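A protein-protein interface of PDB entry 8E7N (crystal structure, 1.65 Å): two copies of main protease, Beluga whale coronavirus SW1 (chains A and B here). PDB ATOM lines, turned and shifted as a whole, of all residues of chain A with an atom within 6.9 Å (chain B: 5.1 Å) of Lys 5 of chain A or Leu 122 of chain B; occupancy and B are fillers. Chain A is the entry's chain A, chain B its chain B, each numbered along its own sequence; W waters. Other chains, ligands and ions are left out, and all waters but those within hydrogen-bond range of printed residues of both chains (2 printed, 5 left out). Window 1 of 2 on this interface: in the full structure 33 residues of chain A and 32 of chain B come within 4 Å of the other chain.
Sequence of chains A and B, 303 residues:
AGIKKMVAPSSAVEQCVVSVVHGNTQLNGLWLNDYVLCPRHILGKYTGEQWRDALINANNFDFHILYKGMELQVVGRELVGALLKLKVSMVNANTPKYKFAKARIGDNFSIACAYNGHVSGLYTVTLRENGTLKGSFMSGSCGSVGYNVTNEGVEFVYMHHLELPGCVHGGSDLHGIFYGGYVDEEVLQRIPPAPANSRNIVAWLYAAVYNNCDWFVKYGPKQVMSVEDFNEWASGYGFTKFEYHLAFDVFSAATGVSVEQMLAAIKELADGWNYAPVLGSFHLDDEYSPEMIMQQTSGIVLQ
O of Val 7 of chain A sits at hydrogen-bond distance from N of Leu 122 of chain B, 2.8 Å away.
N of Leu 122 of chain A lies within hydrogen-bond range of O of Val 7 of chain B.
The side-chain hydroxyl (OG) of Ser 10 of chain A is in hydrogen-bond range of the backbone NH (N) of Ser 10 of chain B (3.0 Å).
The backbone carbonyl oxygen of Thr 124 of chain A lies within hydrogen-bond range of the side-chain amino group of Lys 4 of chain B.
NZ of Lys 4 of chain A sits close to O of Thr 124 of chain B (3.1 Å).
The side-chain amide nitrogen (NE2) of Gln 295 of chain A sits at hydrogen-bond distance from the backbone carbonyl oxygen (O) of Ser 120 of chain B (3.1 Å).
The side-chain amide nitrogen (NE2) of Gln 296 of chain A lies within hydrogen-bond range of the backbone carbonyl oxygen (O) of Lys 4 of chain A, 2.7 Å away.
The backbone carbonyl oxygen (O) of Ala 8 of chain A sits at hydrogen-bond distance from the side-chain hydroxyl (OH) of Tyr 147 of chain A.
The backbone NH of Ser 120 of chain B is in hydrogen-bond range of the backbone carbonyl oxygen of Cys 113 of chain B, at 2.7 Å.
N of Cys 113 of chain B sits at hydrogen-bond distance from O of Gly 121 of chain B, at 2.8 Å.
Lys 4 of chain A touches Tyr 123 of chain B (CB to CG, 3.8 Å).
O of Lys 5 of chain A touches O of Leu 122 of chain B, at 3.6 Å.
Tyr 123 of chain B touches Lys 5 of chain A (CB to O, 3.5 Å).
CA of Gly 121 of chain B touches SD of Met 6 of chain A, at 3.8 Å.
Met 6 of chain A touches Leu 122 of chain B.
Leu 122 of chain B touches Ala 8 of chain A.
CA of Pro 9 of chain A touches OG of Ser 10 of chain B, at 3.7 Å.
CG of Pro 9 of chain A touches O of Val 119 of chain B, 3.4 Å away.
Pro 9 of chain A touches Ser 120 of chain B.
Lys 4 of chain B touches Tyr 123 of chain A (CE to CD1, 3.5 Å).
Lys 5 of chain A touches two residues of chain B.
Of the printed residues of chain A, Leu 122 of chain B touches Lys 5 (3.6 Å), Met 6 (3.5 Å), Val 7 (2.8 Å) and Ala 8 (3.9 Å).
Of the printed residues of chain A, Gly 121 of chain B touches Met 6 (3.8 Å) and Val 7 (3.3 Å).
Printed residues of chain A within 4 Å of Val 7 of chain B: Leu 122 (2.8 Å).
Printed residues of chain B within 4 Å of Lys 4 of chain A: Tyr 123 (3.8 Å) and Thr 124 (3.0 Å).
Of the printed residues of chain A, Thr 124 of chain B touches Lys 4 (3.0 Å).
Printed residues of chain B within 4 Å of Ala 8 of chain A: Leu 122 (3.9 Å).
Ala 112 of chain B touches none of the printed residues of chain A.
The nearest residue of chain B that does not touch Lys 5 of chain A is Lys 4 of chain B (4.4 Å).
Printed residues of chain B that touch a printed residue of chain A: Lys 4, Val 7, Ser 10, Val 119, Ser 120, Gly 121, Leu 122, Tyr 123 and Thr 124.
Among the printed residues, no Asp or Glu carboxylate lies within 4 Å of a Lys or Arg side-chain nitrogen of the other chain.
Lys 4 of chain A touches Thr 124 of chain B, and with the chains exchanged Thr 124 of chain A touches Lys 4 of chain B.
Val 7 of chain A touches Leu 122 of chain B, and with the chains exchanged Leu 122 of chain A touches Val 7 of chain B.
Ala 8 of chain A touches Leu 122 of chain B, but with the chains exchanged Leu 122 of chain A does not touch Ala 8 of chain B (4.1 Å).
Ser 10 of chain A touches its own counterpart, Ser 10 of chain B.
Water W2 bridges OE1 of Glu 287 of chain A (2.9 Å) and NZ of Lys 4 of chain B (3.1 Å).
Water W1 lies within hydrogen-bond range of the side-chain amino group (NZ) of Lys 4 of chain A and the backbone carbonyl oxygen (O) of Thr 124 of chain B.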
ATOM      1  N   ILE A   3      20.899 -13.015  27.309  1.00  0.00           N
ATOM      2  CA  ILE A   3      21.737 -14.035  27.930  1.00  0.00           C
ATOM      3  C   ILE A   3      21.005 -15.365  27.899  1.00  0.00           C
ATOM      4  O   ILE A   3      19.873 -15.488  28.411  1.00  0.00           O
ATOM      5  CB  ILE A   3      22.097 -13.670  29.376  1.00  0.00           C
ATOM      6  CG1 ILE A   3      22.953 -12.405  29.386  1.00  0.00           C
ATOM      7  CG2 ILE A   3      22.784 -14.855  30.062  1.00  0.00           C
ATOM      8  CD1 ILE A   3      24.333 -12.555  28.669  1.00  0.00           C
ATOM      9  N   LYS A   4      21.656 -16.367  27.321  1.00  0.00           N
ATOM     10  CA  LYS A   4      21.108 -17.714  27.241  1.00  0.00           C
ATOM     11  C   LYS A   4      22.164 -18.714  27.640  1.00  0.00           C
ATOM     12  O   LYS A   4      23.360 -18.418  27.606  1.00  0.00           O
ATOM     13  CB  LYS A   4      20.578 -18.049  25.815  1.00  0.00           C
ATOM     14  CG  LYS A   4      19.465 -17.070  25.340  1.00  0.00           C
ATOM     15  CD  LYS A   4      18.166 -17.288  26.107  1.00  0.00           C
ATOM     16  CE  LYS A   4      17.439 -18.425  25.500  1.00  0.00           C
ATOM     17  NZ  LYS A   4      16.029 -18.416  26.071  1.00  0.00           N
ATOM     18  N   LYS A   5      21.695 -19.904  28.010  1.00  0.00           N
ATOM     19  CA  LYS A   5      22.601 -21.045  28.213  1.00  0.00           C
ATOM     20  C   LYS A   5      23.099 -21.539  26.858  1.00  0.00           C
ATOM     21  O   LYS A   5      22.321 -22.082  26.065  1.00  0.00           O
ATOM     22  CB  LYS A   5      21.843 -22.138  28.954  1.00  0.00           C
ATOM     23  CG  LYS A   5      21.573 -21.782  30.437  1.00  0.00           C
ATOM     24  CD  LYS A   5      22.862 -21.833  31.224  1.00  0.00           C
ATOM     25  CE  LYS A   5      22.531 -21.689  32.717  1.00  0.00           C
ATOM     26  NZ  LYS A   5      21.706 -22.858  33.219  1.00  0.00           N
ATOM     27  N   MET A   6      24.373 -21.396  26.577  1.00  0.00           N
ATOM     28  CA  MET A   6      24.852 -21.589  25.215  1.00  0.00           C
ATOM     29  C   MET A   6      25.552 -22.938  25.126  1.00  0.00           C
ATOM     30  O   MET A   6      26.544 -23.180  25.818  1.00  0.00           O
ATOM     31  CB  MET A   6      25.768 -20.448  24.812  1.00  0.00           C
ATOM     32  CG  MET A   6      24.896 -19.185  24.421  1.00  0.00           C
ATOM     33  SD  MET A   6      25.142 -19.085  22.672  1.00  0.00           S
ATOM     34  CE  MET A   6      26.670 -18.439  23.037  1.00  0.00           C
ATOM     35  N   VAL A   7      25.034 -23.803  24.296  1.00  0.00           N
ATOM     36  CA  VAL A   7      25.572 -25.138  24.123  1.00  0.00           C
ATOM     37  C   VAL A   7      26.596 -25.089  22.997  1.00  0.00           C
ATOM     38  O   VAL A   7      26.408 -24.372  21.992  1.00  0.00           O
ATOM     39  CB  VAL A   7      24.418 -26.098  23.763  1.00  0.00           C
ATOM     40  CG1 VAL A   7      24.964 -27.479  23.349  1.00  0.00           C
ATOM     41  CG2 VAL A   7      23.378 -26.137  24.883  1.00  0.00           C
ATOM     42  N   ALA A   8      27.711 -25.945  23.094  1.00  0.00           N
ATOM     43  CA  ALA A   8      28.618 -25.945  21.986  1.00  0.00           C
ATOM     44  C   ALA A   8      28.023 -26.709  20.812  1.00  0.00           C
ATOM     45  O   ALA A   8      27.331 -27.714  21.009  1.00  0.00           O
ATOM     46  CB  ALA A   8      29.941 -26.606  22.435  1.00  0.00           C
ATOM     47  N   PRO A   9      28.295 -26.279  19.573  1.00  0.00           N
ATOM     48  CA  PRO A   9      27.821 -27.037  18.391  1.00  0.00           C
ATOM     49  C   PRO A   9      28.232 -28.513  18.458  1.00  0.00           C
ATOM     50  O   PRO A   9      29.339 -28.867  18.901  1.00  0.00           O
ATOM     51  CB  PRO A   9      28.520 -26.324  17.214  1.00  0.00           C
ATOM     52  CG  PRO A   9      28.873 -24.964  17.787  1.00  0.00           C
ATOM     53  CD  PRO A   9      29.193 -25.165  19.237  1.00  0.00           C
ATOM     54  N   SER A  10      27.342 -29.402  18.009  1.00  0.00           N
ATOM     55  CA  SER A  10      27.517 -30.810  18.330  1.00  0.00           C
ATOM     56  C   SER A  10      28.040 -31.686  17.157  1.00  0.00           C
ATOM     57  O   SER A  10      28.177 -32.909  17.324  1.00  0.00           O
ATOM     58  CB  SER A  10      26.175 -31.364  18.862  1.00  0.00           C
ATOM     59  OG  SER A  10      25.117 -31.324  17.894  1.00  0.00           O
ATOM     60  N   SER A  11      28.233 -31.114  15.976  1.00  0.00           N
ATOM     61  CA  SER A  11      28.569 -31.956  14.800  1.00  0.00           C
ATOM     62  C   SER A  11      29.670 -32.963  15.076  1.00  0.00           C
ATOM     63  O   SER A  11      29.539 -34.133  14.705  1.00  0.00           O
ATOM     64  CB  SER A  11      28.998 -31.090  13.610  1.00  0.00           C
ATOM     65  OG  SER A  11      30.089 -30.235  13.997  1.00  0.00           O
ATOM     66  N   ASN A 108      31.384 -24.423  32.760  1.00  0.00           N
ATOM     67  CA  ASN A 108      30.332 -25.051  31.962  1.00  0.00           C
ATOM     68  C   ASN A 108      30.898 -26.101  31.018  1.00  0.00           C
ATOM     69  O   ASN A 108      32.061 -26.040  30.604  1.00  0.00           O
ATOM     70  CB  ASN A 108      29.639 -24.031  31.091  1.00  0.00           C
ATOM     71  CG  ASN A 108      28.842 -23.016  31.921  1.00  0.00           C
ATOM     72  OD1 ASN A 108      29.076 -21.816  31.744  1.00  0.00           O
ATOM     73  ND2 ASN A 108      27.876 -23.473  32.720  1.00  0.00           N
ATOM     74  N   LEU A 122      20.660 -31.533  23.571  1.00  0.00           N
ATOM     75  CA  LEU A 122      21.835 -31.041  24.259  1.00  0.00           C
ATOM     76  C   LEU A 122      21.445 -29.953  25.240  1.00  0.00           C
ATOM     77  O   LEU A 122      20.424 -29.291  25.077  1.00  0.00           O
ATOM     78  CB  LEU A 122      22.838 -30.492  23.275  1.00  0.00           C
ATOM     79  CG  LEU A 122      23.302 -31.642  22.294  1.00  0.00           C
ATOM     80  CD1 LEU A 122      22.784 -31.153  21.060  1.00  0.00           C
ATOM     81  CD2 LEU A 122      24.797 -31.726  22.279  1.00  0.00           C
ATOM     82  N   TYR A 123      22.286 -29.788  26.253  1.00  0.00           N
ATOM     83  CA  TYR A 123      22.101 -28.703  27.183  1.00  0.00           C
ATOM     84  C   TYR A 123      23.423 -28.433  27.882  1.00  0.00           C
ATOM     85  O   TYR A 123      24.398 -29.179  27.697  1.00  0.00           O
ATOM     86  CB  TYR A 123      20.975 -29.014  28.193  1.00  0.00           C
ATOM     87  CG  TYR A 123      21.131 -30.361  28.899  1.00  0.00           C
ATOM     88  CD1 TYR A 123      21.987 -30.491  29.991  1.00  0.00           C
ATOM     89  CD2 TYR A 123      20.456 -31.505  28.460  1.00  0.00           C
ATOM     90  CE1 TYR A 123      22.153 -31.707  30.652  1.00  0.00           C
ATOM     91  CE2 TYR A 123      20.639 -32.729  29.108  1.00  0.00           C
ATOM     92  CZ  TYR A 123      21.469 -32.832  30.179  1.00  0.00           C
ATOM     93  OH  TYR A 123      21.596 -34.061  30.808  1.00  0.00           O
ATOM     94  N   THR A 124      23.478 -27.306  28.626  1.00  0.00           N
ATOM     95  CA  THR A 124      24.691 -27.002  29.388  1.00  0.00           C
ATOM     96  C   THR A 124      24.540 -27.387  30.852  1.00  0.00           C
ATOM     97  O   THR A 124      23.431 -27.376  31.437  1.00  0.00           O
ATOM     98  CB  THR A 124      25.063 -25.529  29.334  1.00  0.00           C
ATOM     99  OG1 THR A 124      24.095 -24.798  30.092  1.00  0.00           O
ATOM    100  CG2 THR A 124      25.084 -25.085  27.888  1.00  0.00           C
ATOM    101  N   VAL A 125      25.682 -27.722  31.445  1.00  0.00           N
ATOM    102  CA  VAL A 125      25.748 -27.979  32.882  1.00  0.00           C
ATOM    103  C   VAL A 125      26.894 -27.143  33.456  1.00  0.00           C
ATOM    104  O   VAL A 125      27.721 -26.581  32.732  1.00  0.00           O
ATOM    105  CB  VAL A 125      25.940 -29.469  33.249  1.00  0.00           C
ATOM    106  CG1 VAL A 125      24.776 -30.302  32.774  1.00  0.00           C
ATOM    107  CG2 VAL A 125      27.232 -29.998  32.617  1.00  0.00           C
ATOM    108  N   THR A 126      26.973 -27.139  34.770  1.00  0.00           N
ATOM    109  CA  THR A 126      28.037 -26.455  35.512  1.00  0.00           C
ATOM    110  C   THR A 126      28.591 -27.431  36.535  1.00  0.00           C
ATOM    111  O   THR A 126      27.802 -28.096  37.213  1.00  0.00           O
ATOM    112  CB  THR A 126      27.426 -25.267  36.241  1.00  0.00           C
ATOM    113  OG1 THR A 126      26.599 -24.536  35.289  1.00  0.00           O
ATOM    114  CG2 THR A 126      28.521 -24.412  36.737  1.00  0.00           C
ATOM    115  N   TYR A 147      31.195 -32.098  26.817  1.00  0.00           N
ATOM    116  CA  TYR A 147      32.309 -31.682  25.943  1.00  0.00           C
ATOM    117  C   TYR A 147      32.320 -30.171  25.862  1.00  0.00           C
ATOM    118  O   TYR A 147      31.342 -29.488  26.162  1.00  0.00           O
ATOM    119  CB  TYR A 147      32.160 -32.289  24.536  1.00  0.00           C
ATOM    120  CG  TYR A 147      30.965 -31.775  23.794  1.00  0.00           C
ATOM    121  CD1 TYR A 147      29.666 -32.288  24.045  1.00  0.00           C
ATOM    122  CD2 TYR A 147      31.108 -30.713  22.838  1.00  0.00           C
ATOM    123  CE1 TYR A 147      28.546 -31.787  23.385  1.00  0.00           C
ATOM    124  CE2 TYR A 147      29.974 -30.202  22.170  1.00  0.00           C
ATOM    125  CZ  TYR A 147      28.707 -30.759  22.437  1.00  0.00           C
ATOM    126  OH  TYR A 147      27.541 -30.312  21.848  1.00  0.00           O
ATOM    127  N   ASP A 285      22.201 -16.285  40.245  1.00  0.00           N
ATOM    128  CA  ASP A 285      22.367 -17.436  39.359  1.00  0.00           C
ATOM    129  C   ASP A 285      23.854 -17.717  39.266  1.00  0.00           C
ATOM    130  O   ASP A 285      24.637 -16.826  38.873  1.00  0.00           O
ATOM    131  CB  ASP A 285      21.764 -17.152  37.987  1.00  0.00           C
ATOM    132  CG  ASP A 285      21.595 -18.437  37.159  1.00  0.00           C
ATOM    133  OD1 ASP A 285      22.406 -19.359  37.307  1.00  0.00           O
ATOM    134  OD2 ASP A 285      20.587 -18.512  36.437  1.00  0.00           O
ATOM    135  N   ASP A 286      24.249 -18.952  39.648  1.00  0.00           N
ATOM    136  CA  ASP A 286      25.652 -19.351  39.595  1.00  0.00           C
ATOM    137  C   ASP A 286      25.933 -20.319  38.457  1.00  0.00           C
ATOM    138  O   ASP A 286      27.000 -20.934  38.450  1.00  0.00           O
ATOM    139  CB  ASP A 286      26.126 -19.938  40.962  1.00  0.00           C
ATOM    140  CG  ASP A 286      25.740 -21.400  41.192  1.00  0.00           C
ATOM    141  OD1 ASP A 286      24.802 -21.898  40.544  1.00  0.00           O
ATOM    142  OD2 ASP A 286      26.396 -22.016  42.069  1.00  0.00           O
ATOM    143  N   GLU A 287      25.005 -20.492  37.518  1.00  0.00           N
ATOM    144  CA  GLU A 287      25.206 -21.524  36.493  1.00  0.00           C
ATOM    145  C   GLU A 287      25.929 -21.046  35.259  1.00  0.00           C
ATOM    146  O   GLU A 287      26.165 -21.882  34.344  1.00  0.00           O
ATOM    147  CB  GLU A 287      23.878 -22.117  36.099  1.00  0.00           C
ATOM    148  CG  GLU A 287      23.335 -22.891  37.251  1.00  0.00           C
ATOM    149  CD  GLU A 287      21.973 -23.532  36.984  1.00  0.00           C
ATOM    150  OE1 GLU A 287      21.276 -23.211  35.994  1.00  0.00           O
ATOM    151  OE2 GLU A 287      21.680 -24.489  37.722  1.00  0.00           O
ATOM    152  N   TYR A 288      26.296 -19.767  35.176  1.00  0.00           N
ATOM    153  CA  TYR A 288      27.005 -19.265  33.995  1.00  0.00           C
ATOM    154  C   TYR A 288      28.480 -19.047  34.344  1.00  0.00           C
ATOM    155  O   TYR A 288      28.803 -18.215  35.204  1.00  0.00           O
ATOM    156  CB  TYR A 288      26.430 -17.942  33.485  1.00  0.00           C
ATOM    157  CG  TYR A 288      25.031 -17.995  32.975  1.00  0.00           C
ATOM    158  CD1 TYR A 288      23.947 -17.954  33.848  1.00  0.00           C
ATOM    159  CD2 TYR A 288      24.789 -18.078  31.607  1.00  0.00           C
ATOM    160  CE1 TYR A 288      22.635 -18.058  33.390  1.00  0.00           C
ATOM    161  CE2 TYR A 288      23.469 -18.117  31.146  1.00  0.00           C
ATOM    162  CZ  TYR A 288      22.422 -18.097  32.025  1.00  0.00           C
ATOM    163  OH  TYR A 288      21.125 -18.147  31.518  1.00  0.00           O
ATOM    164  N   MET A 292      31.123 -18.348  29.398  1.00  0.00           N
ATOM    165  CA  MET A 292      29.817 -18.290  28.744  1.00  0.00           C
ATOM    166  C   MET A 292      29.246 -16.867  28.694  1.00  0.00           C
ATOM    167  O   MET A 292      28.578 -16.504  27.722  1.00  0.00           O
ATOM    168  CB  MET A 292      28.847 -19.260  29.434  1.00  0.00           C
ATOM    169  CG  MET A 292      27.561 -19.410  28.619  1.00  0.00           C
ATOM    170  SD  MET A 292      26.425 -20.578  29.379  1.00  0.00           S
ATOM    171  CE  MET A 292      27.330 -22.065  28.942  1.00  0.00           C
ATOM    172  N   GLN A 295      31.274 -14.910  25.933  1.00  0.00           N
ATOM    173  CA  GLN A 295      30.933 -15.221  24.559  1.00  0.00           C
ATOM    174  C   GLN A 295      29.664 -14.499  24.128  1.00  0.00           C
ATOM    175  O   GLN A 295      29.395 -14.379  22.918  1.00  0.00           O
ATOM    176  CB  GLN A 295      30.857 -16.762  24.430  1.00  0.00           C
ATOM    177  CG  GLN A 295      30.007 -17.395  23.334  1.00  0.00           C
ATOM    178  CD  GLN A 295      29.720 -18.899  23.542  1.00  0.00           C
ATOM    179  OE1 GLN A 295      29.899 -19.453  24.639  1.00  0.00           O
ATOM    180  NE2 GLN A 295      29.399 -19.583  22.430  1.00  0.00           N
ATOM    181  N   GLN A 296      28.860 -14.034  25.091  1.00  0.00           N
ATOM    182  CA  GLN A 296      27.575 -13.416  24.808  1.00  0.00           C
ATOM    183  C   GLN A 296      27.569 -11.933  25.005  1.00  0.00           C
ATOM    184  O   GLN A 296      26.537 -11.307  24.775  1.00  0.00           O
ATOM    185  CB  GLN A 296      26.471 -14.030  25.690  1.00  0.00           C
ATOM    186  CG  GLN A 296      26.184 -15.411  25.236  1.00  0.00           C
ATOM    187  CD  GLN A 296      25.130 -15.980  26.122  1.00  0.00           C
ATOM    188  OE1 GLN A 296      23.975 -15.652  25.939  1.00  0.00           O
ATOM    189  NE2 GLN A 296      25.511 -16.825  27.086  1.00  0.00           N
ATOM    190  N   LYS B   4      15.931 -29.473  31.867  1.00  0.00           N
ATOM    191  CA  LYS B   4      16.832 -28.519  31.231  1.00  0.00           C
ATOM    192  C   LYS B   4      16.230 -28.047  29.920  1.00  0.00           C
ATOM    193  O   LYS B   4      15.393 -28.726  29.327  1.00  0.00           O
ATOM    194  CB  LYS B   4      18.203 -29.179  30.962  1.00  0.00           C
ATOM    195  CG  LYS B   4      18.851 -29.769  32.190  1.00  0.00           C
ATOM    196  CD  LYS B   4      19.511 -28.721  33.108  1.00  0.00           C
ATOM    197  CE  LYS B   4      20.835 -28.362  32.539  1.00  0.00           C
ATOM    198  NZ  LYS B   4      21.462 -27.225  33.331  1.00  0.00           N
ATOM    199  N   VAL B   7      18.329 -28.410  23.498  1.00  0.00           N
ATOM    200  CA  VAL B   7      18.583 -27.988  22.128  1.00  0.00           C
ATOM    201  C   VAL B   7      18.665 -29.200  21.220  1.00  0.00           C
ATOM    202  O   VAL B   7      19.200 -30.250  21.602  1.00  0.00           O
ATOM    203  CB  VAL B   7      19.928 -27.219  22.083  1.00  0.00           C
ATOM    204  CG1 VAL B   7      20.123 -26.662  20.767  1.00  0.00           C
ATOM    205  CG2 VAL B   7      19.809 -26.049  23.064  1.00  0.00           C
ATOM    206  N   ALA B   8      18.206 -29.042  19.978  1.00  0.00           N
ATOM    207  CA  ALA B   8      18.369 -30.134  19.029  1.00  0.00           C
ATOM    208  C   ALA B   8      19.800 -30.182  18.483  1.00  0.00           C
ATOM    209  O   ALA B   8      20.438 -29.145  18.287  1.00  0.00           O
ATOM    210  CB  ALA B   8      17.420 -29.956  17.844  1.00  0.00           C
ATOM    211  N   SER B  10      23.021 -30.143  16.128  1.00  0.00           N
ATOM    212  CA  SER B  10      23.182 -29.127  15.099  1.00  0.00           C
ATOM    213  C   SER B  10      23.968 -29.602  13.870  1.00  0.00           C
ATOM    214  O   SER B  10      24.221 -28.805  12.974  1.00  0.00           O
ATOM    215  CB  SER B  10      23.845 -27.883  15.699  1.00  0.00           C
ATOM    216  OG  SER B  10      25.140 -28.297  16.189  1.00  0.00           O
ATOM    217  N   ILE B 111      18.183 -22.344  18.297  1.00  0.00           N
ATOM    218  CA  ILE B 111      18.882 -21.315  17.519  1.00  0.00           C
ATOM    219  C   ILE B 111      20.313 -21.787  17.303  1.00  0.00           C
ATOM    220  O   ILE B 111      20.994 -22.150  18.274  1.00  0.00           O
ATOM    221  CB  ILE B 111      18.913 -19.974  18.258  1.00  0.00           C
ATOM    222  CG1 ILE B 111      17.503 -19.376  18.424  1.00  0.00           C
ATOM    223  CG2 ILE B 111      19.910 -19.017  17.559  1.00  0.00           C
ATOM    224  CD1 ILE B 111      16.841 -19.113  17.021  1.00  0.00           C
ATOM    225  N   ALA B 112      20.781 -21.781  16.043  1.00  0.00           N
ATOM    226  CA  ALA B 112      22.190 -22.017  15.722  1.00  0.00           C
ATOM    227  C   ALA B 112      22.807 -20.622  15.581  1.00  0.00           C
ATOM    228  O   ALA B 112      22.855 -20.026  14.477  1.00  0.00           O
ATOM    229  CB  ALA B 112      22.316 -22.855  14.451  1.00  0.00           C
ATOM    230  N   CYS B 113      23.305 -20.102  16.710  1.00  0.00           N
ATOM    231  CA  CYS B 113      23.828 -18.743  16.729  1.00  0.00           C
ATOM    232  C   CYS B 113      25.177 -18.680  16.019  1.00  0.00           C
ATOM    233  O   CYS B 113      26.130 -19.390  16.380  1.00  0.00           O
ATOM    234  CB  CYS B 113      23.951 -18.280  18.185  1.00  0.00           C
ATOM    235  SG  CYS B 113      24.250 -16.489  18.253  1.00  0.00           S
ATOM    236  N   VAL B 119      28.791 -21.467  13.244  1.00  0.00           N
ATOM    237  CA  VAL B 119      27.940 -21.557  14.428  1.00  0.00           C
ATOM    238  C   VAL B 119      28.816 -21.520  15.673  1.00  0.00           C
ATOM    239  O   VAL B 119      29.742 -22.326  15.818  1.00  0.00           O
ATOM    240  CB  VAL B 119      27.079 -22.836  14.391  1.00  0.00           C
ATOM    241  CG1 VAL B 119      26.231 -22.935  15.719  1.00  0.00           C
ATOM    242  CG2 VAL B 119      26.185 -22.835  13.134  1.00  0.00           C
ATOM    243  N   SER B 120      28.523 -20.595  16.591  1.00  0.00           N
ATOM    244  CA  SER B 120      29.313 -20.445  17.798  1.00  0.00           C
ATOM    245  C   SER B 120      28.659 -21.056  19.013  1.00  0.00           C
ATOM    246  O   SER B 120      29.359 -21.469  19.936  1.00  0.00           O
ATOM    247  CB  SER B 120      29.610 -18.979  18.076  1.00  0.00           C
ATOM    248  OG  SER B 120      28.449 -18.230  18.144  1.00  0.00           O
ATOM    249  N   GLY B 121      27.337 -21.153  19.016  1.00  0.00           N
ATOM    250  CA  GLY B 121      26.626 -21.602  20.206  1.00  0.00           C
ATOM    251  C   GLY B 121      25.217 -21.942  19.809  1.00  0.00           C
ATOM    252  O   GLY B 121      24.714 -21.397  18.818  1.00  0.00           O
ATOM    253  N   LEU B 122      24.590 -22.875  20.531  1.00  0.00           N
ATOM    254  CA  LEU B 122      23.185 -23.218  20.319  1.00  0.00           C
ATOM    255  C   LEU B 122      22.380 -22.881  21.568  1.00  0.00           C
ATOM    256  O   LEU B 122      22.906 -22.951  22.671  1.00  0.00           O
ATOM    257  CB  LEU B 122      22.993 -24.720  20.043  1.00  0.00           C
ATOM    258  CG  LEU B 122      24.056 -25.396  19.162  1.00  0.00           C
ATOM    259  CD1 LEU B 122      23.866 -26.963  19.275  1.00  0.00           C
ATOM    260  CD2 LEU B 122      23.834 -24.850  17.747  1.00  0.00           C
ATOM    261  N   TYR B 123      21.101 -22.501  21.392  1.00  0.00           N
ATOM    262  CA  TYR B 123      20.245 -22.361  22.568  1.00  0.00           C
ATOM    263  C   TYR B 123      18.772 -22.500  22.199  1.00  0.00           C
ATOM    264  O   TYR B 123      18.402 -22.445  21.038  1.00  0.00           O
ATOM    265  CB  TYR B 123      20.488 -21.055  23.324  1.00  0.00           C
ATOM    266  CG  TYR B 123      20.420 -19.820  22.470  1.00  0.00           C
ATOM    267  CD1 TYR B 123      19.191 -19.229  22.202  1.00  0.00           C
ATOM    268  CD2 TYR B 123      21.557 -19.250  21.994  1.00  0.00           C
ATOM    269  CE1 TYR B 123      19.055 -18.097  21.367  1.00  0.00           C
ATOM    270  CE2 TYR B 123      21.464 -18.065  21.189  1.00  0.00           C
ATOM    271  CZ  TYR B 123      20.224 -17.522  20.896  1.00  0.00           C
ATOM    272  OH  TYR B 123      20.102 -16.378  20.155  1.00  0.00           O
ATOM    273  N   THR B 124      17.941 -22.740  23.219  1.00  0.00           N
ATOM    274  CA  THR B 124      16.507 -22.887  23.029  1.00  0.00           C
ATOM    275  C   THR B 124      15.823 -21.535  23.092  1.00  0.00           C
ATOM    276  O   THR B 124      16.172 -20.691  23.922  1.00  0.00           O
ATOM    277  CB  THR B 124      15.947 -23.789  24.136  1.00  0.00           C
ATOM    278  OG1 THR B 124      16.538 -25.081  23.948  1.00  0.00           O
ATOM    279  CG2 THR B 124      14.450 -23.974  24.010  1.00  0.00           C
ATOM    280  N   TYR B 147      15.627 -23.905  14.301  1.00  0.00           N
ATOM    281  CA  TYR B 147      15.328 -25.175  13.640  1.00  0.00           C
ATOM    282  C   TYR B 147      14.846 -26.182  14.674  1.00  0.00           C
ATOM    283  O   TYR B 147      15.084 -26.033  15.869  1.00  0.00           O
ATOM    284  CB  TYR B 147      16.595 -25.766  12.922  1.00  0.00           C
ATOM    285  CG  TYR B 147      17.706 -26.132  13.897  1.00  0.00           C
ATOM    286  CD1 TYR B 147      18.554 -25.149  14.405  1.00  0.00           C
ATOM    287  CD2 TYR B 147      17.883 -27.458  14.326  1.00  0.00           C
ATOM    288  CE1 TYR B 147      19.564 -25.429  15.343  1.00  0.00           C
ATOM    289  CE2 TYR B 147      18.914 -27.765  15.227  1.00  0.00           C
ATOM    290  CZ  TYR B 147      19.713 -26.761  15.761  1.00  0.00           C
ATOM    291  OH  TYR B 147      20.687 -26.992  16.718  1.00  0.00           O
HETATM  292  O   HOH W   1      13.265 -20.380  25.810  1.00  0.00           O
HETATM  293  O   HOH W   2      19.882 -25.725  35.604  1.00  0.00           O
